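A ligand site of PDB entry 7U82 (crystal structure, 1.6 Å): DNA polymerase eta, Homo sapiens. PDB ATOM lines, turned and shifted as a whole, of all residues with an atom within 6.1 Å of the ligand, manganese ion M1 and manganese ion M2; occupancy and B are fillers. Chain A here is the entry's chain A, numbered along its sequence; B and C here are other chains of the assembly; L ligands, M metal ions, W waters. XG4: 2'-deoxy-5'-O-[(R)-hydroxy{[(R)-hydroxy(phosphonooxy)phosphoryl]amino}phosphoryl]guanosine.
N of Phe 21 lies within hydrogen-bond range of O3' of the ligand, at 3.0 Å.
The backbone NH (N) of Phe 20 sits at hydrogen-bond distance from an oxygen (O2B) of the ligand, 3.3 Å away.
N3 of DA 5 of chain B lies within hydrogen-bond range of N1 of the ligand (3.1 Å).
O4' of DA 5 of chain B is in hydrogen-bond range of N2 of the ligand, at 3.2 Å.
The side-chain amide oxygen (OE1) of Gln 41 sits at hydrogen-bond distance from a nitrogen (N2) of the ligand, at 3.3 Å.
OH of Tyr 55 is in hydrogen-bond range of O3G of the ligand (2.6 Å).
An oxygen (O3G) of the ligand lies within hydrogen-bond range of the backbone NH (N) of Cys 19 (2.8 Å).
NH2 of Arg 58 lies within salt-bridge range of O1G of the ligand (3.2 Å).
O3G of the ligand is in salt-bridge range of NZ of Lys 234.
The guanidinium group (NH2) of Arg 64 lies within hydrogen-bond range of an oxygen (O6) of the ligand (3.1 Å).
O2 of DT 4 of chain B lies within hydrogen-bond range of a nitrogen (N1) of the ligand (2.6 Å).
An oxygen (O2A) of the ligand sits close to O3' of DT 8 of chain C (2.7 Å).
The backbone NH (N) of Asp 118 sits at hydrogen-bond distance from the side-chain hydroxyl (OG) of Ser 116 (2.9 Å).
The side-chain carboxylate of Asp 16 lies close to the side-chain amino group of Lys 227 (3.7 Å).
The guanidinium group (NE) of Arg 58 is in hydrogen-bond range of the backbone carbonyl oxygen (O) of Val 53, at 3.0 Å.
The guanidinium group (NH2) of Arg 64 sits at hydrogen-bond distance from O4 of DT 4 of chain B.
The backbone NH (N) of Glu 119 sits at hydrogen-bond distance from the side-chain hydroxyl (OG) of Ser 116.
The guanidinium group of Arg 64 lies within hydrogen-bond range of O4 of DT 3 of chain B, at 2.7 Å.
NZ of Lys 234 sits at hydrogen-bond distance from O of Asp 16 (3.2 Å).
The side-chain amino group (NZ) of Lys 234 lies close to the backbone carbonyl oxygen (O) of Met 17 (3.4 Å).
Asp 18 touches the ligand (CA to O3G, 3.3 Å).
O of Ile 51 touches C2' of the ligand, at 3.5 Å.
Ala 52 touches the ligand.
Leu 92 touches the ligand.
CG2 of Ile 117 touches O4' of the ligand, at 3.9 Å.
DT 3 of chain B touches the ligand (O4 to O6, 3.8 Å).
Hydrophobic or aromatic side chains within 4 Å of the ligand: Phe 20, Phe 21, Ile 51, Ala 52, Tyr 55, Leu 92 and Ile 117.
Of the 26 residues printed, 20 come within 4 Å of the ligand.
Residues that only touch manganese ion M1: Ser 116 (3.8 Å).
Of the 26 residues printed, 4 come within 4 Å of manganese ion M1.
Along chain A the residues within 4 Å of manganese ion M1 span positions 16 to 119.
Lys 234 touches manganese ion M2.
Of the 26 residues printed, 4 come within 4 Å of manganese ion M2.
Manganese ion M1 is bound by the side-chain carboxylate of Asp 118 (2.0 Å), water W4 (2.1 Å), the side-chain carboxylate of Asp 16 (2.2 Å), the side-chain carboxylate of Glu 119 (2.2 Å), an oxygen (O1A) of the ligand (2.3 Å) and water W3 (2.3 Å).
The side-chain carboxylate (OD1) of Asp 16 is bound to manganese ion M2, 2.1 Å away.
Manganese ion M2 is bound by O of Met 17 (2.1 Å).
Manganese ion M2 is bound by OD2 of Asp 118, 2.1 Å away.
O2G of the ligand binds manganese ion M2, 2.2 Å away.
Manganese ion M2 is bound by O1B of the ligand (2.2 Å).
O1A of the ligand binds manganese ion M2 (2.3 Å).
Water W4 lies within hydrogen-bond range of O5' of the ligand (3.3 Å) and OG of Ser 116 (3.3 Å).
Water W3 lies within hydrogen-bond range of NZ of Lys 227 (2.9 Å) and O2A of the ligand (3.2 Å).
Water W1 lies within hydrogen-bond range of O2B of the ligand (2.7 Å), N of Val 53 (2.8 Å) and NH2 of Arg 58 (2.9 Å).
Water W6 bridges N3A of the ligand (3.0 Å) and O of Ile 51 (3.1 Å).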
ATOM      1  N   ASP A  16      11.103  21.294  -5.675  1.00  0.00           N
ATOM      2  CA  ASP A  16       9.734  20.840  -5.381  1.00  0.00           C
ATOM      3  C   ASP A  16       9.198  20.021  -6.556  1.00  0.00           C
ATOM      4  O   ASP A  16       9.187  20.527  -7.672  1.00  0.00           O
ATOM      5  CB  ASP A  16       8.809  22.013  -5.148  1.00  0.00           C
ATOM      6  CG  ASP A  16       7.434  21.576  -4.736  1.00  0.00           C
ATOM      7  OD1 ASP A  16       6.633  21.299  -5.611  1.00  0.00           O
ATOM      8  OD2 ASP A  16       7.187  21.557  -3.527  1.00  0.00           O
ATOM      9  N   MET A  17       8.742  18.818  -6.249  1.00  0.00           N
ATOM     10  CA  MET A  17       8.267  17.931  -7.334  1.00  0.00           C
ATOM     11  C   MET A  17       6.993  18.500  -7.961  1.00  0.00           C
ATOM     12  O   MET A  17       6.128  18.980  -7.252  1.00  0.00           O
ATOM     13  CB  MET A  17       8.026  16.519  -6.813  1.00  0.00           C
ATOM     14  CG  MET A  17       9.197  15.938  -6.050  1.00  0.00           C
ATOM     15  SD  MET A  17      10.721  15.971  -7.001  1.00  0.00           S
ATOM     16  CE  MET A  17      10.278  14.919  -8.364  1.00  0.00           C
ATOM     17  N   ASP A  18       6.911  18.450  -9.279  1.00  0.00           N
ATOM     18  CA  ASP A  18       5.689  18.919  -9.965  1.00  0.00           C
ATOM     19  C   ASP A  18       4.552  17.932  -9.745  1.00  0.00           C
ATOM     20  O   ASP A  18       4.781  16.744  -9.892  1.00  0.00           O
ATOM     21  CB  ASP A  18       5.944  19.120 -11.458  1.00  0.00           C
ATOM     22  CG  ASP A  18       7.030  20.123 -11.784  1.00  0.00           C
ATOM     23  OD1 ASP A  18       7.194  21.086 -11.037  1.00  0.00           O
ATOM     24  OD2 ASP A  18       7.692  19.924 -12.799  1.00  0.00           O
ATOM     25  N   CYS A  19       3.368  18.436  -9.406  1.00  0.00           N
ATOM     26  CA  CYS A  19       2.168  17.627  -9.145  1.00  0.00           C
ATOM     27  C   CYS A  19       2.503  16.204  -8.658  1.00  0.00           C
ATOM     28  O   CYS A  19       2.146  15.221  -9.321  1.00  0.00           O
ATOM     29  CB  CYS A  19       1.254  17.628 -10.396  1.00  0.00           C
ATOM     30  SG  CYS A  19       1.935  17.202 -11.968  1.00  0.00           S
ATOM     31  N   PHE A  20       3.179  16.109  -7.510  1.00  0.00           N
ATOM     32  CA  PHE A  20       3.951  14.901  -7.176  1.00  0.00           C
ATOM     33  C   PHE A  20       3.112  13.618  -7.198  1.00  0.00           C
ATOM     34  O   PHE A  20       3.484  12.634  -7.855  1.00  0.00           O
ATOM     35  CB  PHE A  20       4.626  15.077  -5.806  1.00  0.00           C
ATOM     36  CG  PHE A  20       5.510  13.918  -5.419  1.00  0.00           C
ATOM     37  CD1 PHE A  20       6.432  13.411  -6.326  1.00  0.00           C
ATOM     38  CD2 PHE A  20       5.422  13.341  -4.164  1.00  0.00           C
ATOM     39  CE1 PHE A  20       7.276  12.347  -5.977  1.00  0.00           C
ATOM     40  CE2 PHE A  20       6.236  12.279  -3.827  1.00  0.00           C
ATOM     41  CZ  PHE A  20       7.162  11.790  -4.726  1.00  0.00           C
ATOM     42  N   PHE A  21       1.996  13.571  -6.450  1.00  0.00           N
ATOM     43  CA  PHE A  21       1.272  12.299  -6.412  1.00  0.00           C
ATOM     44  C   PHE A  21       0.765  11.905  -7.796  1.00  0.00           C
ATOM     45  O   PHE A  21       0.679  10.709  -8.118  1.00  0.00           O
ATOM     46  CB  PHE A  21       0.082  12.314  -5.434  1.00  0.00           C
ATOM     47  CG  PHE A  21       0.448  12.344  -3.960  1.00  0.00           C
ATOM     48  CD1 PHE A  21       1.715  12.676  -3.503  1.00  0.00           C
ATOM     49  CD2 PHE A  21      -0.542  12.021  -3.023  1.00  0.00           C
ATOM     50  CE1 PHE A  21       1.982  12.713  -2.112  1.00  0.00           C
ATOM     51  CE2 PHE A  21      -0.276  12.032  -1.652  1.00  0.00           C
ATOM     52  CZ  PHE A  21       0.979  12.383  -1.201  1.00  0.00           C
ATOM     53  N   VAL A  22       0.390  12.907  -8.627  1.00  0.00           N
ATOM     54  CA  VAL A  22       0.006  12.607  -9.992  1.00  0.00           C
ATOM     55  C   VAL A  22       1.171  11.980 -10.747  1.00  0.00           C
ATOM     56  O   VAL A  22       0.994  10.972 -11.436  1.00  0.00           O
ATOM     57  CB  VAL A  22      -0.502  13.881 -10.699  1.00  0.00           C
ATOM     58  CG1 VAL A  22      -0.535  13.680 -12.210  1.00  0.00           C
ATOM     59  CG2 VAL A  22      -1.888  14.228 -10.168  1.00  0.00           C
ATOM     60  N   GLN A  41      -8.592  11.130  -2.683  1.00  0.00           N
ATOM     61  CA  GLN A  41      -8.730  10.185  -1.582  1.00  0.00           C
ATOM     62  C   GLN A  41     -10.206   9.882  -1.358  1.00  0.00           C
ATOM     63  O   GLN A  41     -11.032  10.802  -1.298  1.00  0.00           O
ATOM     64  CB  GLN A  41      -8.051  10.638  -0.278  1.00  0.00           C
ATOM     65  CG  GLN A  41      -6.829  11.519  -0.437  1.00  0.00           C
ATOM     66  CD  GLN A  41      -6.243  11.978   0.909  1.00  0.00           C
ATOM     67  OE1 GLN A  41      -5.324  11.355   1.436  1.00  0.00           O
ATOM     68  NE2 GLN A  41      -6.776  13.071   1.442  1.00  0.00           N
ATOM     69  N   ILE A  51      -6.353  15.871  -4.137  1.00  0.00           N
ATOM     70  CA  ILE A  51      -5.186  16.387  -3.429  1.00  0.00           C
ATOM     71  C   ILE A  51      -4.030  16.729  -4.354  1.00  0.00           C
ATOM     72  O   ILE A  51      -3.072  17.354  -3.892  1.00  0.00           O
ATOM     73  CB  ILE A  51      -4.715  15.417  -2.324  1.00  0.00           C
ATOM     74  CG1 ILE A  51      -4.449  14.007  -2.877  1.00  0.00           C
ATOM     75  CG2 ILE A  51      -5.681  15.439  -1.141  1.00  0.00           C
ATOM     76  CD1 ILE A  51      -3.763  13.073  -1.874  1.00  0.00           C
ATOM     77  N   ALA A  52      -4.096  16.398  -5.657  1.00  0.00           N
ATOM     78  CA  ALA A  52      -3.014  16.689  -6.577  1.00  0.00           C
ATOM     79  C   ALA A  52      -3.579  16.718  -7.992  1.00  0.00           C
ATOM     80  O   ALA A  52      -4.469  15.928  -8.302  1.00  0.00           O
ATOM     81  CB  ALA A  52      -1.889  15.647  -6.490  1.00  0.00           C
ATOM     82  N   VAL A  53      -3.062  17.629  -8.834  1.00  0.00           N
ATOM     83  CA  VAL A  53      -3.673  17.933 -10.131  1.00  0.00           C
ATOM     84  C   VAL A  53      -2.591  18.150 -11.188  1.00  0.00           C
ATOM     85  O   VAL A  53      -1.706  18.987 -11.004  1.00  0.00           O
ATOM     86  CB  VAL A  53      -4.580  19.181 -10.052  1.00  0.00           C
ATOM     87  CG1 VAL A  53      -5.303  19.389 -11.346  1.00  0.00           C
ATOM     88  CG2 VAL A  53      -5.575  19.031  -8.946  1.00  0.00           C
ATOM     89  N   TYR A  55      -0.863  19.510 -14.625  1.00  0.00           N
ATOM     90  CA  TYR A  55      -0.945  20.863 -15.180  1.00  0.00           C
ATOM     91  C   TYR A  55      -1.958  20.943 -16.324  1.00  0.00           C
ATOM     92  O   TYR A  55      -2.631  21.984 -16.493  1.00  0.00           O
ATOM     93  CB  TYR A  55       0.453  21.308 -15.597  1.00  0.00           C
ATOM     94  CG  TYR A  55       1.212  21.733 -14.352  1.00  0.00           C
ATOM     95  CD1 TYR A  55       1.770  20.797 -13.497  1.00  0.00           C
ATOM     96  CD2 TYR A  55       1.299  23.077 -14.007  1.00  0.00           C
ATOM     97  CE1 TYR A  55       2.442  21.180 -12.335  1.00  0.00           C
ATOM     98  CE2 TYR A  55       1.957  23.484 -12.864  1.00  0.00           C
ATOM     99  CZ  TYR A  55       2.512  22.530 -12.018  1.00  0.00           C
ATOM    100  OH  TYR A  55       3.172  22.946 -10.870  1.00  0.00           O
ATOM    101  N   ARG A  58      -5.156  21.412 -14.519  1.00  0.00           N
ATOM    102  CA  ARG A  58      -5.228  22.747 -13.939  1.00  0.00           C
ATOM    103  C   ARG A  58      -5.719  23.763 -14.958  1.00  0.00           C
ATOM    104  O   ARG A  58      -6.387  24.735 -14.580  1.00  0.00           O
ATOM    105  CB  ARG A  58      -3.864  23.193 -13.413  1.00  0.00           C
ATOM    106  CG  ARG A  58      -3.326  22.324 -12.321  1.00  0.00           C
ATOM    107  CD  ARG A  58      -2.038  22.900 -11.791  1.00  0.00           C
ATOM    108  NE  ARG A  58      -1.412  21.940 -10.897  1.00  0.00           N
ATOM    109  CZ  ARG A  58      -0.427  22.223 -10.066  1.00  0.00           C
ATOM    110  NH1 ARG A  58       0.087  23.446 -10.000  1.00  0.00           N
ATOM    111  NH2 ARG A  58       0.032  21.266  -9.260  1.00  0.00           N
ATOM    112  N   ARG A  64      -6.581  21.335  -6.073  1.00  0.00           N
ATOM    113  CA  ARG A  64      -6.660  20.609  -4.818  1.00  0.00           C
ATOM    114  C   ARG A  64      -7.809  21.174  -3.984  1.00  0.00           C
ATOM    115  O   ARG A  64      -8.214  22.325  -4.154  1.00  0.00           O
ATOM    116  CB  ARG A  64      -5.314  20.674  -4.063  1.00  0.00           C
ATOM    117  CG  ARG A  64      -5.109  21.845  -3.128  1.00  0.00           C
ATOM    118  CD  ARG A  64      -3.865  21.687  -2.219  1.00  0.00           C
ATOM    119  NE  ARG A  64      -4.126  21.078  -0.918  1.00  0.00           N
ATOM    120  CZ  ARG A  64      -4.651  21.733   0.106  1.00  0.00           C
ATOM    121  NH1 ARG A  64      -5.023  23.003   0.005  1.00  0.00           N
ATOM    122  NH2 ARG A  64      -4.821  21.102   1.280  1.00  0.00           N
ATOM    123  N   LEU A  92      -0.700   6.335   2.405  1.00  0.00           N
ATOM    124  CA  LEU A  92       0.148   7.116   1.508  1.00  0.00           C
ATOM    125  C   LEU A  92       1.541   6.516   1.311  1.00  0.00           C
ATOM    126  O   LEU A  92       2.459   7.216   0.879  1.00  0.00           O
ATOM    127  CB  LEU A  92       0.249   8.556   2.006  1.00  0.00           C
ATOM    128  CG  LEU A  92      -1.094   9.223   2.301  1.00  0.00           C
ATOM    129  CD1 LEU A  92      -0.933  10.602   2.875  1.00  0.00           C
ATOM    130  CD2 LEU A  92      -1.946   9.210   1.045  1.00  0.00           C
ATOM    131  N   SER A 116       8.969  18.697   3.065  1.00  0.00           N
ATOM    132  CA  SER A 116       7.671  18.050   2.949  1.00  0.00           C
ATOM    133  C   SER A 116       7.898  16.744   2.214  1.00  0.00           C
ATOM    134  O   SER A 116       9.023  16.407   1.864  1.00  0.00           O
ATOM    135  CB  SER A 116       6.689  18.915   2.172  1.00  0.00           C
ATOM    136  OG  SER A 116       6.930  18.695   0.795  1.00  0.00           O
ATOM    137  N   ILE A 117       6.808  16.004   1.958  1.00  0.00           N
ATOM    138  CA  ILE A 117       6.917  14.792   1.159  1.00  0.00           C
ATOM    139  C   ILE A 117       7.493  15.050  -0.222  1.00  0.00           C
ATOM    140  O   ILE A 117       8.036  14.128  -0.840  1.00  0.00           O
ATOM    141  CB  ILE A 117       5.525  14.125   1.064  1.00  0.00           C
ATOM    142  CG1 ILE A 117       5.664  12.677   0.622  1.00  0.00           C
ATOM    143  CG2 ILE A 117       4.627  14.916   0.128  1.00  0.00           C
ATOM    144  CD1 ILE A 117       4.381  11.909   0.862  1.00  0.00           C
ATOM    145  N   ASP A 118       7.376  16.264  -0.746  1.00  0.00           N
ATOM    146  CA  ASP A 118       7.850  16.400  -2.122  1.00  0.00           C
ATOM    147  C   ASP A 118       8.818  17.559  -2.326  1.00  0.00           C
ATOM    148  O   ASP A 118       9.046  17.972  -3.474  1.00  0.00           O
ATOM    149  CB  ASP A 118       6.692  16.538  -3.110  1.00  0.00           C
ATOM    150  CG  ASP A 118       6.272  17.951  -3.351  1.00  0.00           C
ATOM    151  OD1 ASP A 118       6.246  18.768  -2.400  1.00  0.00           O
ATOM    152  OD2 ASP A 118       6.034  18.248  -4.548  1.00  0.00           O
ATOM    153  N   GLU A 119       9.420  18.082  -1.257  1.00  0.00           N
ATOM    154  CA  GLU A 119      10.344  19.160  -1.504  1.00  0.00           C
ATOM    155  C   GLU A 119      11.395  19.218  -0.415  1.00  0.00           C
ATOM    156  O   GLU A 119      11.144  18.828   0.746  1.00  0.00           O
ATOM    157  CB  GLU A 119       9.639  20.508  -1.589  1.00  0.00           C
ATOM    158  CG  GLU A 119       9.269  21.027  -0.226  1.00  0.00           C
ATOM    159  CD  GLU A 119       8.041  21.849  -0.290  1.00  0.00           C
ATOM    160  OE1 GLU A 119       6.947  21.262  -0.433  1.00  0.00           O
ATOM    161  OE2 GLU A 119       8.166  23.095  -0.175  1.00  0.00           O
ATOM    162  N   LYS A 227      12.079  29.271  -2.103  1.00  0.00           N
ATOM    163  CA  LYS A 227      10.732  28.693  -2.245  1.00  0.00           C
ATOM    164  C   LYS A 227       9.878  29.531  -3.186  1.00  0.00           C
ATOM    165  O   LYS A 227       9.185  29.003  -4.093  1.00  0.00           O
ATOM    166  CB  LYS A 227      10.091  28.593  -0.855  1.00  0.00           C
ATOM    167  CG  LYS A 227       8.633  28.116  -0.855  1.00  0.00           C
ATOM    168  CD  LYS A 227       8.505  26.671  -1.377  1.00  0.00           C
ATOM    169  CE  LYS A 227       7.032  26.206  -1.347  1.00  0.00           C
ATOM    170  NZ  LYS A 227       6.799  24.799  -1.843  1.00  0.00           N
ATOM    171  N   LYS A 234       6.827  27.142 -12.582  1.00  0.00           N
ATOM    172  CA  LYS A 234       6.391  25.726 -12.666  1.00  0.00           C
ATOM    173  C   LYS A 234       5.497  25.547 -13.903  1.00  0.00           C
ATOM    174  O   LYS A 234       4.754  26.470 -14.224  1.00  0.00           O
ATOM    175  CB  LYS A 234       5.610  25.370 -11.401  1.00  0.00           C
ATOM    176  CG  LYS A 234       6.423  25.102 -10.150  1.00  0.00           C
ATOM    177  CD  LYS A 234       5.627  24.354  -9.107  1.00  0.00           C
ATOM    178  CE  LYS A 234       6.497  23.554  -8.158  1.00  0.00           C
ATOM    179  NZ  LYS A 234       6.482  22.096  -8.467  1.00  0.00           N
ATOM    180  N   PRO A 235       5.484  24.384 -14.568  1.00  0.00           N
ATOM    181  CA  PRO A 235       6.329  23.247 -14.183  1.00  0.00           C
ATOM    182  C   PRO A 235       7.636  23.001 -14.942  1.00  0.00           C
ATOM    183  O   PRO A 235       7.874  23.656 -15.906  1.00  0.00           O
ATOM    184  CB  PRO A 235       5.398  22.086 -14.547  1.00  0.00           C
ATOM    185  CG  PRO A 235       4.711  22.539 -15.807  1.00  0.00           C
ATOM    186  CD  PRO A 235       4.603  24.045 -15.684  1.00  0.00           C
ATOM    187  P    DT B   3     -16.883  20.431   3.371  1.00  0.00           P
ATOM    188  OP1  DT B   3     -17.725  21.374   4.140  1.00  0.00           O
ATOM    189  OP2  DT B   3     -16.730  20.602   1.904  1.00  0.00           O
ATOM    190  O5'  DT B   3     -15.455  20.431   4.074  1.00  0.00           O
ATOM    191  C5'  DT B   3     -14.249  20.320   3.299  1.00  0.00           C
ATOM    192  C4'  DT B   3     -13.952  18.871   3.016  1.00  0.00           C
ATOM    193  O4'  DT B   3     -12.936  18.791   1.982  1.00  0.00           O
ATOM    194  C3'  DT B   3     -13.387  18.098   4.206  1.00  0.00           C
ATOM    195  O3'  DT B   3     -13.781  16.724   4.154  1.00  0.00           O
ATOM    196  C2'  DT B   3     -11.898  18.193   3.985  1.00  0.00           C
ATOM    197  C1'  DT B   3     -11.833  18.045   2.476  1.00  0.00           C
ATOM    198  N1   DT B   3     -10.605  18.609   1.917  1.00  0.00           N
ATOM    199  C2   DT B   3      -9.771  17.788   1.182  1.00  0.00           C
ATOM    200  O2   DT B   3     -10.035  16.629   0.930  1.00  0.00           O
ATOM    201  N3   DT B   3      -8.624  18.401   0.737  1.00  0.00           N
ATOM    202  C4   DT B   3      -8.231  19.699   0.958  1.00  0.00           C
ATOM    203  O4   DT B   3      -7.176  20.106   0.495  1.00  0.00           O
ATOM    204  C5   DT B   3      -9.148  20.493   1.749  1.00  0.00           C
ATOM    205  C7   DT B   3      -8.802  21.918   2.064  1.00  0.00           C
ATOM    206  C6   DT B   3     -10.269  19.913   2.183  1.00  0.00           C
ATOM    207  P    DT B   4     -13.352  15.714   5.322  1.00  0.00           P
ATOM    208  OP1  DT B   4     -14.260  14.553   5.269  1.00  0.00           O
ATOM    209  OP2  DT B   4     -13.178  16.484   6.564  1.00  0.00           O
ATOM    210  O5'  DT B   4     -11.899  15.251   4.887  1.00  0.00           O
ATOM    211  C5'  DT B   4     -11.672  14.432   3.747  1.00  0.00           C
ATOM    212  C4'  DT B   4     -10.286  13.855   3.828  1.00  0.00           C
ATOM    213  O4'  DT B   4      -9.312  14.827   3.386  1.00  0.00           O
ATOM    214  C3'  DT B   4      -9.849  13.456   5.236  1.00  0.00           C
ATOM    215  O3'  DT B   4      -9.156  12.228   5.033  1.00  0.00           O
ATOM    216  C2'  DT B   4      -8.948  14.596   5.663  1.00  0.00           C
ATOM    217  C1'  DT B   4      -8.299  14.982   4.359  1.00  0.00           C
ATOM    218  N1   DT B   4      -7.839  16.367   4.270  1.00  0.00           N
ATOM    219  C2   DT B   4      -6.727  16.602   3.510  1.00  0.00           C
ATOM    220  O2   DT B   4      -6.075  15.708   2.990  1.00  0.00           O
ATOM    221  N3   DT B   4      -6.366  17.926   3.416  1.00  0.00           N
ATOM    222  C4   DT B   4      -7.036  19.009   3.924  1.00  0.00           C
ATOM    223  O4   DT B   4      -6.573  20.133   3.790  1.00  0.00           O
ATOM    224  C5   DT B   4      -8.183  18.690   4.742  1.00  0.00           C
ATOM    225  C7   DT B   4      -8.931  19.804   5.404  1.00  0.00           C
ATOM    226  C6   DT B   4      -8.542  17.406   4.847  1.00  0.00           C
ATOM    227  P    DA B   5      -8.507  11.459   6.242  1.00  0.00           P
ATOM    228  OP1  DA B   5      -8.813  10.033   6.080  1.00  0.00           O
ATOM    229  OP2  DA B   5      -8.862  12.131   7.480  1.00  0.00           O
ATOM    230  O5'  DA B   5      -6.951  11.686   6.015  1.00  0.00           O
ATOM    231  C5'  DA B   5      -6.320  11.253   4.813  1.00  0.00           C
ATOM    232  C4'  DA B   5      -4.839  11.510   4.888  1.00  0.00           C
ATOM    233  O4'  DA B   5      -4.599  12.929   4.754  1.00  0.00           O
ATOM    234  C3'  DA B   5      -4.189  11.086   6.204  1.00  0.00           C
ATOM    235  O3'  DA B   5      -2.899  10.552   5.921  1.00  0.00           O
ATOM    236  C2'  DA B   5      -4.116  12.397   6.981  1.00  0.00           C
ATOM    237  C1'  DA B   5      -3.861  13.394   5.871  1.00  0.00           C
ATOM    238  N9   DA B   5      -4.310  14.749   6.176  1.00  0.00           N
ATOM    239  C8   DA B   5      -5.400  15.129   6.912  1.00  0.00           C
ATOM    240  N7   DA B   5      -5.556  16.422   6.985  1.00  0.00           N
ATOM    241  C5   DA B   5      -4.507  16.938   6.236  1.00  0.00           C
ATOM    242  C6   DA B   5      -4.121  18.243   5.919  1.00  0.00           C
ATOM    243  N6   DA B   5      -4.759  19.331   6.349  1.00  0.00           N
ATOM    244  N1   DA B   5      -3.017  18.404   5.149  1.00  0.00           N
ATOM    245  C2   DA B   5      -2.371  17.312   4.724  1.00  0.00           C
ATOM    246  N3   DA B   5      -2.641  16.036   4.959  1.00  0.00           N
ATOM    247  C4   DA B   5      -3.733  15.909   5.722  1.00  0.00           C
ATOM    248  P    DT C   8       1.890  26.284   0.944  1.00  0.00           P
ATOM    249  OP1  DT C   8       3.084  26.489   0.101  1.00  0.00           O
ATOM    250  OP2  DT C   8       0.821  27.316   0.997  1.00  0.00           O
ATOM    251  O5'  DT C   8       1.220  24.906   0.512  1.00  0.00           O
ATOM    252  C5'  DT C   8       1.916  23.658   0.653  1.00  0.00           C
ATOM    253  C4'  DT C   8       0.948  22.520   0.436  1.00  0.00           C
ATOM    254  O4'  DT C   8       0.277  22.189   1.681  1.00  0.00           O
ATOM    255  C3'  DT C   8      -0.163  22.811  -0.570  1.00  0.00           C
ATOM    256  O3'  DT C   8      -0.435  21.685  -1.392  1.00  0.00           O
ATOM    257  C2'  DT C   8      -1.380  23.018   0.297  1.00  0.00           C
ATOM    258  C1'  DT C   8      -1.079  21.970   1.347  1.00  0.00           C
ATOM    259  N1   DT C   8      -1.879  22.073   2.556  1.00  0.00           N
ATOM    260  C2   DT C   8      -1.998  20.961   3.342  1.00  0.00           C
ATOM    261  O2   DT C   8      -1.381  19.930   3.121  1.00  0.00           O
ATOM    262  N3   DT C   8      -2.836  21.098   4.421  1.00  0.00           N
ATOM    263  C4   DT C   8      -3.573  22.208   4.759  1.00  0.00           C
ATOM    264  O4   DT C   8      -4.286  22.180   5.758  1.00  0.00           O
ATOM    265  C5   DT C   8      -3.438  23.340   3.871  1.00  0.00           C
ATOM    266  C7   DT C   8      -4.200  24.588   4.167  1.00  0.00           C
ATOM    267  C6   DT C   8      -2.615  23.215   2.823  1.00  0.00           C
HETATM  268  N1  XG4 L   1      -3.668  16.009   2.010  1.00  0.00           N
HETATM  269  C2  XG4 L   1      -2.856  15.009   1.561  1.00  0.00           C
HETATM  270  N2  XG4 L   1      -3.113  13.791   2.034  1.00  0.00           N
HETATM  271  N3  XG4 L   1      -1.874  15.135   0.665  1.00  0.00           N
HETATM  272  C4  XG4 L   1      -1.718  16.377   0.220  1.00  0.00           C
HETATM  273  C5  XG4 L   1      -2.444  17.455   0.573  1.00  0.00           C
HETATM  274  C6  XG4 L   1      -3.478  17.244   1.511  1.00  0.00           C
HETATM  275  O6  XG4 L   1      -4.231  18.168   1.873  1.00  0.00           O
HETATM  276  N7  XG4 L   1      -2.000  18.597  -0.091  1.00  0.00           N
HETATM  277  C8  XG4 L   1      -1.001  18.166  -0.836  1.00  0.00           C
HETATM  278  N9  XG4 L   1      -0.783  16.818  -0.697  1.00  0.00           N
HETATM  279  PA  XG4 L   1       2.577  20.201  -3.363  1.00  0.00           P
HETATM  280  PB  XG4 L   1       2.076  19.299  -6.124  1.00  0.00           P
HETATM  281  PG  XG4 L   1       3.020  21.560  -7.609  1.00  0.00           P
HETATM  282  C1' XG4 L   1       0.170  15.954  -1.406  1.00  0.00           C
HETATM  283  O1A XG4 L   1       4.010  20.392  -3.637  1.00  0.00           O
HETATM  284  O1B XG4 L   1       3.391  18.653  -5.999  1.00  0.00           O
HETATM  285  O1G XG4 L   1       2.201  22.843  -7.606  1.00  0.00           O
HETATM  286  C2' XG4 L   1      -0.163  15.747  -2.880  1.00  0.00           C
HETATM  287  O2A XG4 L   1       1.940  21.414  -2.585  1.00  0.00           O
HETATM  288  O2B XG4 L   1       0.945  18.269  -6.387  1.00  0.00           O
HETATM  289  O2G XG4 L   1       4.088  21.518  -6.530  1.00  0.00           O
HETATM  290  C3' XG4 L   1       0.860  16.605  -3.598  1.00  0.00           C
HETATM  291  O3' XG4 L   1       1.159  16.001  -4.855  1.00  0.00           O
HETATM  292  N3A XG4 L   1       1.681  20.047  -4.729  1.00  0.00           N
HETATM  293  O3B XG4 L   1       2.030  20.359  -7.274  1.00  0.00           O
HETATM  294  O3G XG4 L   1       3.614  21.213  -8.956  1.00  0.00           O
HETATM  295  C4' XG4 L   1       2.050  16.559  -2.656  1.00  0.00           C
HETATM  296  O4' XG4 L   1       1.466  16.558  -1.341  1.00  0.00           O
HETATM  297  C5' XG4 L   1       3.035  17.696  -2.770  1.00  0.00           C
HETATM  298  O5' XG4 L   1       2.323  18.926  -2.463  1.00  0.00           O
HETATM  299 MN    MN M   1       5.696  20.715  -2.176  1.00  0.00          MN
HETATM  300 MN    MN M   2       5.145  19.868  -5.604  1.00  0.00          MN
HETATM  301  O   HOH W   1      -1.258  19.292  -7.588  1.00  0.00           O
HETATM  302  O   HOH W   2      -0.041  23.356  -6.326  1.00  0.00           O
HETATM  303  O   HOH W   3       4.773  22.809  -2.261  1.00  0.00           O
HETATM  304  O   HOH W   4       4.449  20.442  -0.474  1.00  0.00           O
HETATM  305  O   HOH W   5       4.605  23.733  -4.915  1.00  0.00           O
HETATM  306  O   HOH W   6      -1.265  19.789  -4.235  1.00  0.00           O
